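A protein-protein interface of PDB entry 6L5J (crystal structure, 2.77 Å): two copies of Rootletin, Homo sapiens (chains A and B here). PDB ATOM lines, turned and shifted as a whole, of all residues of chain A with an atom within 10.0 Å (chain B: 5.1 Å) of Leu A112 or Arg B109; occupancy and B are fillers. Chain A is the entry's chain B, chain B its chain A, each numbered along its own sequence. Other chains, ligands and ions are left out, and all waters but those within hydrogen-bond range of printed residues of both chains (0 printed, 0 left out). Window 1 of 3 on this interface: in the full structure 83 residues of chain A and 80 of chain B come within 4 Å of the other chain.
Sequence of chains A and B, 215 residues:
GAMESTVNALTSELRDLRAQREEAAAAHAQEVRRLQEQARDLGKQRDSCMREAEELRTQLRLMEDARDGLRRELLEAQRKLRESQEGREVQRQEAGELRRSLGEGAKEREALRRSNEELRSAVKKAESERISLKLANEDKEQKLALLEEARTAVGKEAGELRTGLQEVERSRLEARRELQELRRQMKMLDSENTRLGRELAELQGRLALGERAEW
OE2 of Glu B108 lies within salt-bridge range of NH2 of Arg A109, at 3.1 Å. NH1 of Arg B109 lies within salt-bridge range of OE1 of Glu A108, 2.9 Å away.
The guanidinium group of Arg B109 lies close to the backbone carbonyl oxygen of Gly B105.
Among the printed residues, pairs that only touch across the chains: Gly A105 with Arg B109, Asn A116 with Asn B116, Arg A113 with Leu B112, Leu A119 with Asn B116, Leu A112 with Asn B116, Leu A112 with Arg B109, Asn A116 with Leu B112 and Leu A112 with Arg B113.
Leu A112 touches three residues of chain B. Arg B109 touches just these residues of chain A: Gly A105 (3.1 Å), Glu A108 (2.9 Å) and Leu A112 (3.6 Å). No residue of chain A comes within 4 Å of Ala B106. No residue of chain A comes within 4 Å of Glu B110. Of the printed residues of chain A, Asn B116 touches Leu A112, Asn A116 and Leu A119. Of the printed residues of chain B, Glu A108 touches Arg B109 (2.9 Å). Of the printed residues of chain B, Gly A105 touches Arg B109 (3.1 Å). Of the printed residues of chain B, Asn A116 touches Leu B112 and Asn B116. The nearest residue of chain B that does not touch Leu A112 is Leu B112 (4.4 Å). The nearest printed residue of chain B that does not touch Arg A113 is Glu B108 (4.7 Å).
Of the 11 printed residues of chain B, 5 touch a printed residue of chain A. Hydrophobic or aromatic side chains of chain B within 4 Å of the printed part of chain A: Leu B112. Of the 20 printed residues of chain A, 7 touch a printed residue of chain B. Among the printed residues, Asp or Glu carboxylates within 4 Å of a Lys or Arg side-chain nitrogen of the other chain: Glu A108 with Arg B109 (2.9 Å) and Arg A109 with Glu B108 (3.1 Å).
Gly A105 touches Arg B109, but with the chains exchanged Arg A109 does not touch Gly B105 (5.6 Å). Glu A108 touches Arg B109, and with the chains exchanged Arg A109 touches Glu B108. Leu A112 touches Arg B109, but with the chains exchanged Arg A109 does not touch Leu B112 (4.8 Å). Leu A112 touches Arg B113, and with the chains exchanged Arg A113 touches Leu B112. Positions printed for both chains: 104, 105, 106, 107, 108, 109, 110, 111, 112, 113 and 116.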
ATOM      1  N   SER A 101      -5.749 -24.313  -4.543  1.00  0.00           N
ATOM      2  CA  SER A 101      -4.537 -24.960  -4.065  1.00  0.00           C
ATOM      3  C   SER A 101      -3.497 -25.080  -5.172  1.00  0.00           C
ATOM      4  O   SER A 101      -2.297 -25.166  -4.888  1.00  0.00           O
ATOM      5  CB  SER A 101      -4.885 -26.330  -3.480  1.00  0.00           C
ATOM      6  OG  SER A 101      -5.463 -27.165  -4.471  1.00  0.00           O
ATOM      7  N   LEU A 102      -3.933 -25.077  -6.432  1.00  0.00           N
ATOM      8  CA  LEU A 102      -2.997 -25.185  -7.539  1.00  0.00           C
ATOM      9  C   LEU A 102      -2.208 -23.888  -7.700  1.00  0.00           C
ATOM     10  O   LEU A 102      -1.007 -23.911  -8.010  1.00  0.00           O
ATOM     11  CB  LEU A 102      -3.753 -25.514  -8.820  1.00  0.00           C
ATOM     12  CG  LEU A 102      -3.000 -26.113 -10.001  1.00  0.00           C
ATOM     13  CD1 LEU A 102      -2.594 -27.544  -9.685  1.00  0.00           C
ATOM     14  CD2 LEU A 102      -3.803 -26.052 -11.294  1.00  0.00           C
ATOM     15  N   GLY A 103      -2.874 -22.747  -7.493  1.00  0.00           N
ATOM     16  CA  GLY A 103      -2.197 -21.466  -7.572  1.00  0.00           C
ATOM     17  C   GLY A 103      -1.330 -21.202  -6.361  1.00  0.00           C
ATOM     18  O   GLY A 103      -0.223 -20.665  -6.485  1.00  0.00           O
ATOM     19  N   GLU A 104      -1.797 -21.591  -5.173  1.00  0.00           N
ATOM     20  CA  GLU A 104      -0.908 -21.463  -4.027  1.00  0.00           C
ATOM     21  C   GLU A 104       0.213 -22.492  -4.089  1.00  0.00           C
ATOM     22  O   GLU A 104       1.273 -22.277  -3.492  1.00  0.00           O
ATOM     23  CB  GLU A 104      -1.679 -21.599  -2.720  1.00  0.00           C
ATOM     24  CG  GLU A 104      -1.984 -23.011  -2.332  1.00  0.00           C
ATOM     25  CD  GLU A 104      -2.978 -23.088  -1.196  1.00  0.00           C
ATOM     26  OE1 GLU A 104      -3.538 -22.029  -0.817  1.00  0.00           O
ATOM     27  OE2 GLU A 104      -3.191 -24.208  -0.680  1.00  0.00           O
ATOM     28  N   GLY A 105       0.010 -23.591  -4.812  1.00  0.00           N
ATOM     29  CA  GLY A 105       1.098 -24.519  -5.053  1.00  0.00           C
ATOM     30  C   GLY A 105       2.134 -23.973  -6.018  1.00  0.00           C
ATOM     31  O   GLY A 105       3.318 -24.293  -5.912  1.00  0.00           O
ATOM     32  N   ALA A 106       1.710 -23.156  -6.982  1.00  0.00           N
ATOM     33  CA  ALA A 106       2.683 -22.497  -7.841  1.00  0.00           C
ATOM     34  C   ALA A 106       3.221 -21.216  -7.213  1.00  0.00           C
ATOM     35  O   ALA A 106       4.145 -20.613  -7.765  1.00  0.00           O
ATOM     36  CB  ALA A 106       2.082 -22.200  -9.211  1.00  0.00           C
ATOM     37  N   LYS A 107       2.651 -20.789  -6.081  1.00  0.00           N
ATOM     38  CA  LYS A 107       3.211 -19.689  -5.299  1.00  0.00           C
ATOM     39  C   LYS A 107       4.208 -20.193  -4.261  1.00  0.00           C
ATOM     40  O   LYS A 107       5.070 -19.429  -3.812  1.00  0.00           O
ATOM     41  CB  LYS A 107       2.084 -18.910  -4.609  1.00  0.00           C
ATOM     42  CG  LYS A 107       2.514 -17.659  -3.813  1.00  0.00           C
ATOM     43  CD  LYS A 107       1.290 -17.011  -3.145  1.00  0.00           C
ATOM     44  CE  LYS A 107       1.655 -15.809  -2.274  1.00  0.00           C
ATOM     45  NZ  LYS A 107       2.057 -14.630  -3.089  1.00  0.00           N
ATOM     46  N   GLU A 108       4.076 -21.457  -3.841  1.00  0.00           N
ATOM     47  CA  GLU A 108       5.130 -22.111  -3.073  1.00  0.00           C
ATOM     48  C   GLU A 108       6.226 -22.618  -3.998  1.00  0.00           C
ATOM     49  O   GLU A 108       7.372 -22.752  -3.574  1.00  0.00           O
ATOM     50  CB  GLU A 108       4.580 -23.302  -2.263  1.00  0.00           C
ATOM     51  CG  GLU A 108       3.413 -23.020  -1.288  1.00  0.00           C
ATOM     52  CD  GLU A 108       2.975 -24.247  -0.450  1.00  0.00           C
ATOM     53  OE1 GLU A 108       3.564 -25.346  -0.593  1.00  0.00           O
ATOM     54  OE2 GLU A 108       2.023 -24.105   0.352  1.00  0.00           O
ATOM     55  N   ARG A 109       5.880 -22.957  -5.245  1.00  0.00           N
ATOM     56  CA  ARG A 109       6.888 -23.406  -6.199  1.00  0.00           C
ATOM     57  C   ARG A 109       7.818 -22.273  -6.595  1.00  0.00           C
ATOM     58  O   ARG A 109       8.961 -22.514  -6.999  1.00  0.00           O
ATOM     59  CB  ARG A 109       6.236 -23.991  -7.443  1.00  0.00           C
ATOM     60  CG  ARG A 109       7.228 -24.421  -8.512  1.00  0.00           C
ATOM     61  CD  ARG A 109       6.514 -24.982  -9.718  1.00  0.00           C
ATOM     62  NE  ARG A 109       7.428 -25.334 -10.802  1.00  0.00           N
ATOM     63  CZ  ARG A 109       7.023 -25.837 -11.964  1.00  0.00           C
ATOM     64  NH1 ARG A 109       5.729 -26.030 -12.173  1.00  0.00           N
ATOM     65  NH2 ARG A 109       7.896 -26.139 -12.916  1.00  0.00           N
ATOM     66  N   GLU A 110       7.348 -21.028  -6.508  1.00  0.00           N
ATOM     67  CA  GLU A 110       8.247 -19.924  -6.811  1.00  0.00           C
ATOM     68  C   GLU A 110       9.157 -19.611  -5.624  1.00  0.00           C
ATOM     69  O   GLU A 110      10.380 -19.493  -5.788  1.00  0.00           O
ATOM     70  CB  GLU A 110       7.454 -18.698  -7.267  1.00  0.00           C
ATOM     71  CG  GLU A 110       6.861 -18.919  -8.632  1.00  0.00           C
ATOM     72  CD  GLU A 110       7.908 -19.210  -9.707  1.00  0.00           C
ATOM     73  OE1 GLU A 110       8.934 -18.516  -9.769  1.00  0.00           O
ATOM     74  OE2 GLU A 110       7.732 -20.200 -10.456  1.00  0.00           O
ATOM     75  N   ALA A 111       8.588 -19.528  -4.413  1.00  0.00           N
ATOM     76  CA  ALA A 111       9.396 -19.268  -3.225  1.00  0.00           C
ATOM     77  C   ALA A 111      10.549 -20.253  -3.113  1.00  0.00           C
ATOM     78  O   ALA A 111      11.681 -19.857  -2.808  1.00  0.00           O
ATOM     79  CB  ALA A 111       8.530 -19.307  -1.962  1.00  0.00           C
ATOM     80  N   LEU A 112      10.289 -21.534  -3.389  1.00  0.00           N
ATOM     81  CA  LEU A 112      11.336 -22.542  -3.251  1.00  0.00           C
ATOM     82  C   LEU A 112      12.365 -22.461  -4.378  1.00  0.00           C
ATOM     83  O   LEU A 112      13.576 -22.487  -4.111  1.00  0.00           O
ATOM     84  CB  LEU A 112      10.729 -23.939  -3.158  1.00  0.00           C
ATOM     85  CG  LEU A 112      10.455 -24.429  -1.734  1.00  0.00           C
ATOM     86  CD1 LEU A 112       9.377 -23.613  -1.017  1.00  0.00           C
ATOM     87  CD2 LEU A 112      10.083 -25.907  -1.763  1.00  0.00           C
ATOM     88  N   ARG A 113      11.929 -22.350  -5.636  1.00  0.00           N
ATOM     89  CA  ARG A 113      12.919 -22.188  -6.698  1.00  0.00           C
ATOM     90  C   ARG A 113      13.707 -20.894  -6.555  1.00  0.00           C
ATOM     91  O   ARG A 113      14.801 -20.791  -7.114  1.00  0.00           O
ATOM     92  CB  ARG A 113      12.270 -22.245  -8.081  1.00  0.00           C
ATOM     93  CG  ARG A 113      11.857 -23.630  -8.499  1.00  0.00           C
ATOM     94  CD  ARG A 113      11.031 -23.620  -9.776  1.00  0.00           C
ATOM     95  NE  ARG A 113      11.795 -23.278 -10.970  1.00  0.00           N
ATOM     96  CZ  ARG A 113      11.237 -23.010 -12.147  1.00  0.00           C
ATOM     97  NH1 ARG A 113       9.916 -23.035 -12.271  1.00  0.00           N
ATOM     98  NH2 ARG A 113      11.990 -22.712 -13.196  1.00  0.00           N
ATOM     99  N   ARG A 114      13.190 -19.912  -5.813  1.00  0.00           N
ATOM    100  CA  ARG A 114      13.949 -18.688  -5.607  1.00  0.00           C
ATOM    101  C   ARG A 114      14.929 -18.850  -4.447  1.00  0.00           C
ATOM    102  O   ARG A 114      16.094 -18.446  -4.551  1.00  0.00           O
ATOM    103  CB  ARG A 114      13.000 -17.498  -5.396  1.00  0.00           C
ATOM    104  CG  ARG A 114      13.706 -16.153  -5.270  1.00  0.00           C
ATOM    105  CD  ARG A 114      14.398 -15.717  -6.573  1.00  0.00           C
ATOM    106  NE  ARG A 114      15.239 -14.525  -6.376  1.00  0.00           N
ATOM    107  CZ  ARG A 114      16.522 -14.568  -6.011  1.00  0.00           C
ATOM    108  NH1 ARG A 114      17.107 -15.739  -5.821  1.00  0.00           N
ATOM    109  NH2 ARG A 114      17.221 -13.454  -5.833  1.00  0.00           N
ATOM    110  N   SER A 115      14.504 -19.466  -3.341  1.00  0.00           N
ATOM    111  CA  SER A 115      15.483 -19.751  -2.293  1.00  0.00           C
ATOM    112  C   SER A 115      16.484 -20.805  -2.734  1.00  0.00           C
ATOM    113  O   SER A 115      17.584 -20.868  -2.186  1.00  0.00           O
ATOM    114  CB  SER A 115      14.795 -20.195  -1.002  1.00  0.00           C
ATOM    115  OG  SER A 115      14.057 -19.131  -0.431  1.00  0.00           O
ATOM    116  N   ASN A 116      16.121 -21.628  -3.714  1.00  0.00           N
ATOM    117  CA  ASN A 116      17.053 -22.609  -4.246  1.00  0.00           C
ATOM    118  C   ASN A 116      18.213 -21.925  -4.948  1.00  0.00           C
ATOM    119  O   ASN A 116      19.376 -22.290  -4.745  1.00  0.00           O
ATOM    120  CB  ASN A 116      16.321 -23.550  -5.200  1.00  0.00           C
ATOM    121  CG  ASN A 116      17.133 -24.763  -5.555  1.00  0.00           C
ATOM    122  OD1 ASN A 116      18.259 -24.894  -5.120  1.00  0.00           O
ATOM    123  ND2 ASN A 116      16.564 -25.660  -6.346  1.00  0.00           N
ATOM    124  N   GLU A 117      17.924 -20.918  -5.766  1.00  0.00           N
ATOM    125  CA  GLU A 117      19.032 -20.185  -6.359  1.00  0.00           C
ATOM    126  C   GLU A 117      19.749 -19.297  -5.356  1.00  0.00           C
ATOM    127  O   GLU A 117      20.938 -19.033  -5.531  1.00  0.00           O
ATOM    128  CB  GLU A 117      18.578 -19.366  -7.559  1.00  0.00           C
ATOM    129  CG  GLU A 117      18.407 -20.215  -8.800  1.00  0.00           C
ATOM    130  CD  GLU A 117      19.704 -20.908  -9.203  1.00  0.00           C
ATOM    131  OE1 GLU A 117      20.797 -20.352  -8.942  1.00  0.00           O
ATOM    132  OE2 GLU A 117      19.631 -22.013  -9.783  1.00  0.00           O
ATOM    133  N   GLU A 118      19.078 -18.844  -4.298  1.00  0.00           N
ATOM    134  CA  GLU A 118      19.811 -18.105  -3.279  1.00  0.00           C
ATOM    135  C   GLU A 118      20.852 -18.992  -2.590  1.00  0.00           C
ATOM    136  O   GLU A 118      21.928 -18.508  -2.205  1.00  0.00           O
ATOM    137  CB  GLU A 118      18.860 -17.482  -2.255  1.00  0.00           C
ATOM    138  CG  GLU A 118      18.075 -16.292  -2.778  1.00  0.00           C
ATOM    139  CD  GLU A 118      17.272 -15.613  -1.685  1.00  0.00           C
ATOM    140  OE1 GLU A 118      17.279 -16.133  -0.551  1.00  0.00           O
ATOM    141  OE2 GLU A 118      16.642 -14.565  -1.950  1.00  0.00           O
ATOM    142  N   LEU A 119      20.571 -20.290  -2.455  1.00  0.00           N
ATOM    143  CA  LEU A 119      21.537 -21.207  -1.853  1.00  0.00           C
ATOM    144  C   LEU A 119      22.717 -21.462  -2.784  1.00  0.00           C
ATOM    145  O   LEU A 119      23.874 -21.310  -2.379  1.00  0.00           O
ATOM    146  CB  LEU A 119      20.845 -22.518  -1.488  1.00  0.00           C
ATOM    147  CG  LEU A 119      19.779 -22.226  -0.432  1.00  0.00           C
ATOM    148  CD1 LEU A 119      18.932 -23.441  -0.037  1.00  0.00           C
ATOM    149  CD2 LEU A 119      20.454 -21.568   0.769  1.00  0.00           C
ATOM    150  N   ARG A 120      22.437 -21.846  -4.033  1.00  0.00           N
ATOM    151  CA  ARG A 120      23.495 -22.021  -5.018  1.00  0.00           C
ATOM    152  C   ARG A 120      24.306 -20.745  -5.217  1.00  0.00           C
ATOM    153  O   ARG A 120      25.527 -20.816  -5.393  1.00  0.00           O
ATOM    154  CB  ARG A 120      22.885 -22.503  -6.330  1.00  0.00           C
ATOM    155  CG  ARG A 120      22.433 -23.950  -6.258  1.00  0.00           C
ATOM    156  CD  ARG A 120      21.666 -24.394  -7.492  1.00  0.00           C
ATOM    157  NE  ARG A 120      21.317 -25.811  -7.411  1.00  0.00           N
ATOM    158  CZ  ARG A 120      20.450 -26.423  -8.211  1.00  0.00           C
ATOM    159  NH1 ARG A 120      19.798 -25.737  -9.147  1.00  0.00           N
ATOM    160  NH2 ARG A 120      20.214 -27.720  -8.053  1.00  0.00           N
ATOM    161  N   GLU B 104       1.526 -33.663  -9.767  1.00  0.00           N
ATOM    162  CA  GLU B 104       2.872 -33.517 -10.313  1.00  0.00           C
ATOM    163  C   GLU B 104       3.603 -32.349  -9.660  1.00  0.00           C
ATOM    164  O   GLU B 104       4.708 -32.512  -9.124  1.00  0.00           O
ATOM    165  CB  GLU B 104       2.803 -33.322 -11.829  1.00  0.00           C
ATOM    166  CG  GLU B 104       2.174 -34.482 -12.597  1.00  0.00           C
ATOM    167  CD  GLU B 104       2.998 -35.759 -12.519  1.00  0.00           C
ATOM    168  OE1 GLU B 104       4.245 -35.665 -12.412  1.00  0.00           O
ATOM    169  OE2 GLU B 104       2.395 -36.855 -12.571  1.00  0.00           O
ATOM    170  N   GLY B 105       2.987 -31.168  -9.691  1.00  0.00           N
ATOM    171  CA  GLY B 105       3.475 -30.045  -8.925  1.00  0.00           C
ATOM    172  C   GLY B 105       3.748 -30.356  -7.469  1.00  0.00           C
ATOM    173  O   GLY B 105       4.564 -29.675  -6.849  1.00  0.00           O
ATOM    174  N   ALA B 106       3.080 -31.360  -6.898  1.00  0.00           N
ATOM    175  CA  ALA B 106       3.383 -31.721  -5.518  1.00  0.00           C
ATOM    176  C   ALA B 106       4.668 -32.520  -5.441  1.00  0.00           C
ATOM    177  O   ALA B 106       5.455 -32.348  -4.502  1.00  0.00           O
ATOM    178  CB  ALA B 106       2.236 -32.505  -4.893  1.00  0.00           C
ATOM    179  N   LYS B 107       4.913 -33.390  -6.422  1.00  0.00           N
ATOM    180  CA  LYS B 107       6.194 -34.092  -6.430  1.00  0.00           C
ATOM    181  C   LYS B 107       7.357 -33.123  -6.654  1.00  0.00           C
ATOM    182  O   LYS B 107       8.417 -33.268  -6.031  1.00  0.00           O
ATOM    183  CB  LYS B 107       6.207 -35.204  -7.483  1.00  0.00           C
ATOM    184  CG  LYS B 107       5.394 -36.415  -7.105  1.00  0.00           C
ATOM    185  CD  LYS B 107       5.396 -37.431  -8.235  1.00  0.00           C
ATOM    186  CE  LYS B 107       4.424 -38.566  -7.983  1.00  0.00           C
ATOM    187  NZ  LYS B 107       4.517 -39.539  -9.097  1.00  0.00           N
ATOM    188  N   GLU B 108       7.182 -32.126  -7.526  1.00  0.00           N
ATOM    189  CA  GLU B 108       8.280 -31.206  -7.802  1.00  0.00           C
ATOM    190  C   GLU B 108       8.572 -30.324  -6.598  1.00  0.00           C
ATOM    191  O   GLU B 108       9.737 -30.156  -6.225  1.00  0.00           O
ATOM    192  CB  GLU B 108       7.979 -30.364  -9.034  1.00  0.00           C
ATOM    193  CG  GLU B 108       9.139 -29.480  -9.451  1.00  0.00           C
ATOM    194  CD  GLU B 108       8.862 -28.728 -10.731  1.00  0.00           C
ATOM    195  OE1 GLU B 108       7.756 -28.904 -11.287  1.00  0.00           O
ATOM    196  OE2 GLU B 108       9.743 -27.963 -11.173  1.00  0.00           O
ATOM    197  N   ARG B 109       7.541 -29.780  -5.957  1.00  0.00           N
ATOM    198  CA  ARG B 109       7.766 -28.997  -4.746  1.00  0.00           C
ATOM    199  C   ARG B 109       8.447 -29.816  -3.658  1.00  0.00           C
ATOM    200  O   ARG B 109       9.210 -29.267  -2.860  1.00  0.00           O
ATOM    201  CB  ARG B 109       6.454 -28.424  -4.213  1.00  0.00           C
ATOM    202  CG  ARG B 109       5.792 -27.386  -5.137  1.00  0.00           C
ATOM    203  CD  ARG B 109       4.450 -26.884  -4.587  1.00  0.00           C
ATOM    204  NE  ARG B 109       3.513 -27.991  -4.429  1.00  0.00           N
ATOM    205  CZ  ARG B 109       3.056 -28.403  -3.247  1.00  0.00           C
ATOM    206  NH1 ARG B 109       3.436 -27.775  -2.138  1.00  0.00           N
ATOM    207  NH2 ARG B 109       2.224 -29.436  -3.164  1.00  0.00           N
ATOM    208  N   GLU B 110       8.211 -31.122  -3.605  1.00  0.00           N
ATOM    209  CA  GLU B 110       8.855 -31.882  -2.542  1.00  0.00           C
ATOM    210  C   GLU B 110      10.300 -32.207  -2.896  1.00  0.00           C
ATOM    211  O   GLU B 110      11.158 -32.264  -2.007  1.00  0.00           O
ATOM    212  CB  GLU B 110       8.067 -33.155  -2.249  1.00  0.00           C
ATOM    213  CG  GLU B 110       8.503 -33.897  -0.988  1.00  0.00           C
ATOM    214  CD  GLU B 110       8.252 -33.099   0.287  1.00  0.00           C
ATOM    215  OE1 GLU B 110       7.428 -32.161   0.274  1.00  0.00           O
ATOM    216  OE2 GLU B 110       8.851 -33.432   1.329  1.00  0.00           O
ATOM    217  N   ALA B 111      10.595 -32.407  -4.184  1.00  0.00           N
ATOM    218  CA  ALA B 111      11.972 -32.676  -4.592  1.00  0.00           C
ATOM    219  C   ALA B 111      12.848 -31.446  -4.390  1.00  0.00           C
ATOM    220  O   ALA B 111      13.991 -31.555  -3.923  1.00  0.00           O
ATOM    221  CB  ALA B 111      12.011 -33.137  -6.047  1.00  0.00           C
ATOM    222  N   LEU B 112      12.321 -30.266  -4.728  1.00  0.00           N
ATOM    223  CA  LEU B 112      13.025 -29.024  -4.444  1.00  0.00           C
ATOM    224  C   LEU B 112      13.167 -28.806  -2.945  1.00  0.00           C
ATOM    225  O   LEU B 112      14.221 -28.360  -2.475  1.00  0.00           O
ATOM    226  CB  LEU B 112      12.286 -27.847  -5.082  1.00  0.00           C
ATOM    227  CG  LEU B 112      12.199 -27.836  -6.608  1.00  0.00           C
ATOM    228  CD1 LEU B 112      11.372 -26.665  -7.050  1.00  0.00           C
ATOM    229  CD2 LEU B 112      13.577 -27.789  -7.245  1.00  0.00           C
ATOM    230  N   ARG B 113      12.113 -29.099  -2.175  1.00  0.00           N
ATOM    231  CA  ARG B 113      12.224 -28.973  -0.726  1.00  0.00           C
ATOM    232  C   ARG B 113      13.376 -29.821  -0.207  1.00  0.00           C
ATOM    233  O   ARG B 113      14.137 -29.382   0.662  1.00  0.00           O
ATOM    234  CB  ARG B 113      10.903 -29.354  -0.059  1.00  0.00           C
ATOM    235  CG  ARG B 113      10.788 -29.049   1.442  1.00  0.00           C
ATOM    236  CD  ARG B 113      11.120 -30.259   2.315  1.00  0.00           C
ATOM    237  NE  ARG B 113      10.675 -30.073   3.697  1.00  0.00           N
ATOM    238  CZ  ARG B 113      11.005 -30.868   4.712  1.00  0.00           C
ATOM    239  NH1 ARG B 113      11.817 -31.902   4.521  1.00  0.00           N
ATOM    240  NH2 ARG B 113      10.551 -30.610   5.930  1.00  0.00           N
ATOM    241  N   ASN B 116      16.770 -27.806  -1.352  1.00  0.00           N
ATOM    242  CA  ASN B 116      17.145 -26.722  -0.452  1.00  0.00           C
ATOM    243  C   ASN B 116      17.722 -27.259   0.853  1.00  0.00           C
ATOM    244  O   ASN B 116      18.634 -26.650   1.427  1.00  0.00           O
ATOM    245  CB  ASN B 116      15.943 -25.825  -0.143  1.00  0.00           C
ATOM    246  CG  ASN B 116      15.304 -25.236  -1.386  1.00  0.00           C
ATOM    247  OD1 ASN B 116      15.954 -24.966  -2.394  1.00  0.00           O
ATOM    248  ND2 ASN B 116      14.011 -25.000  -1.299  1.00  0.00           N
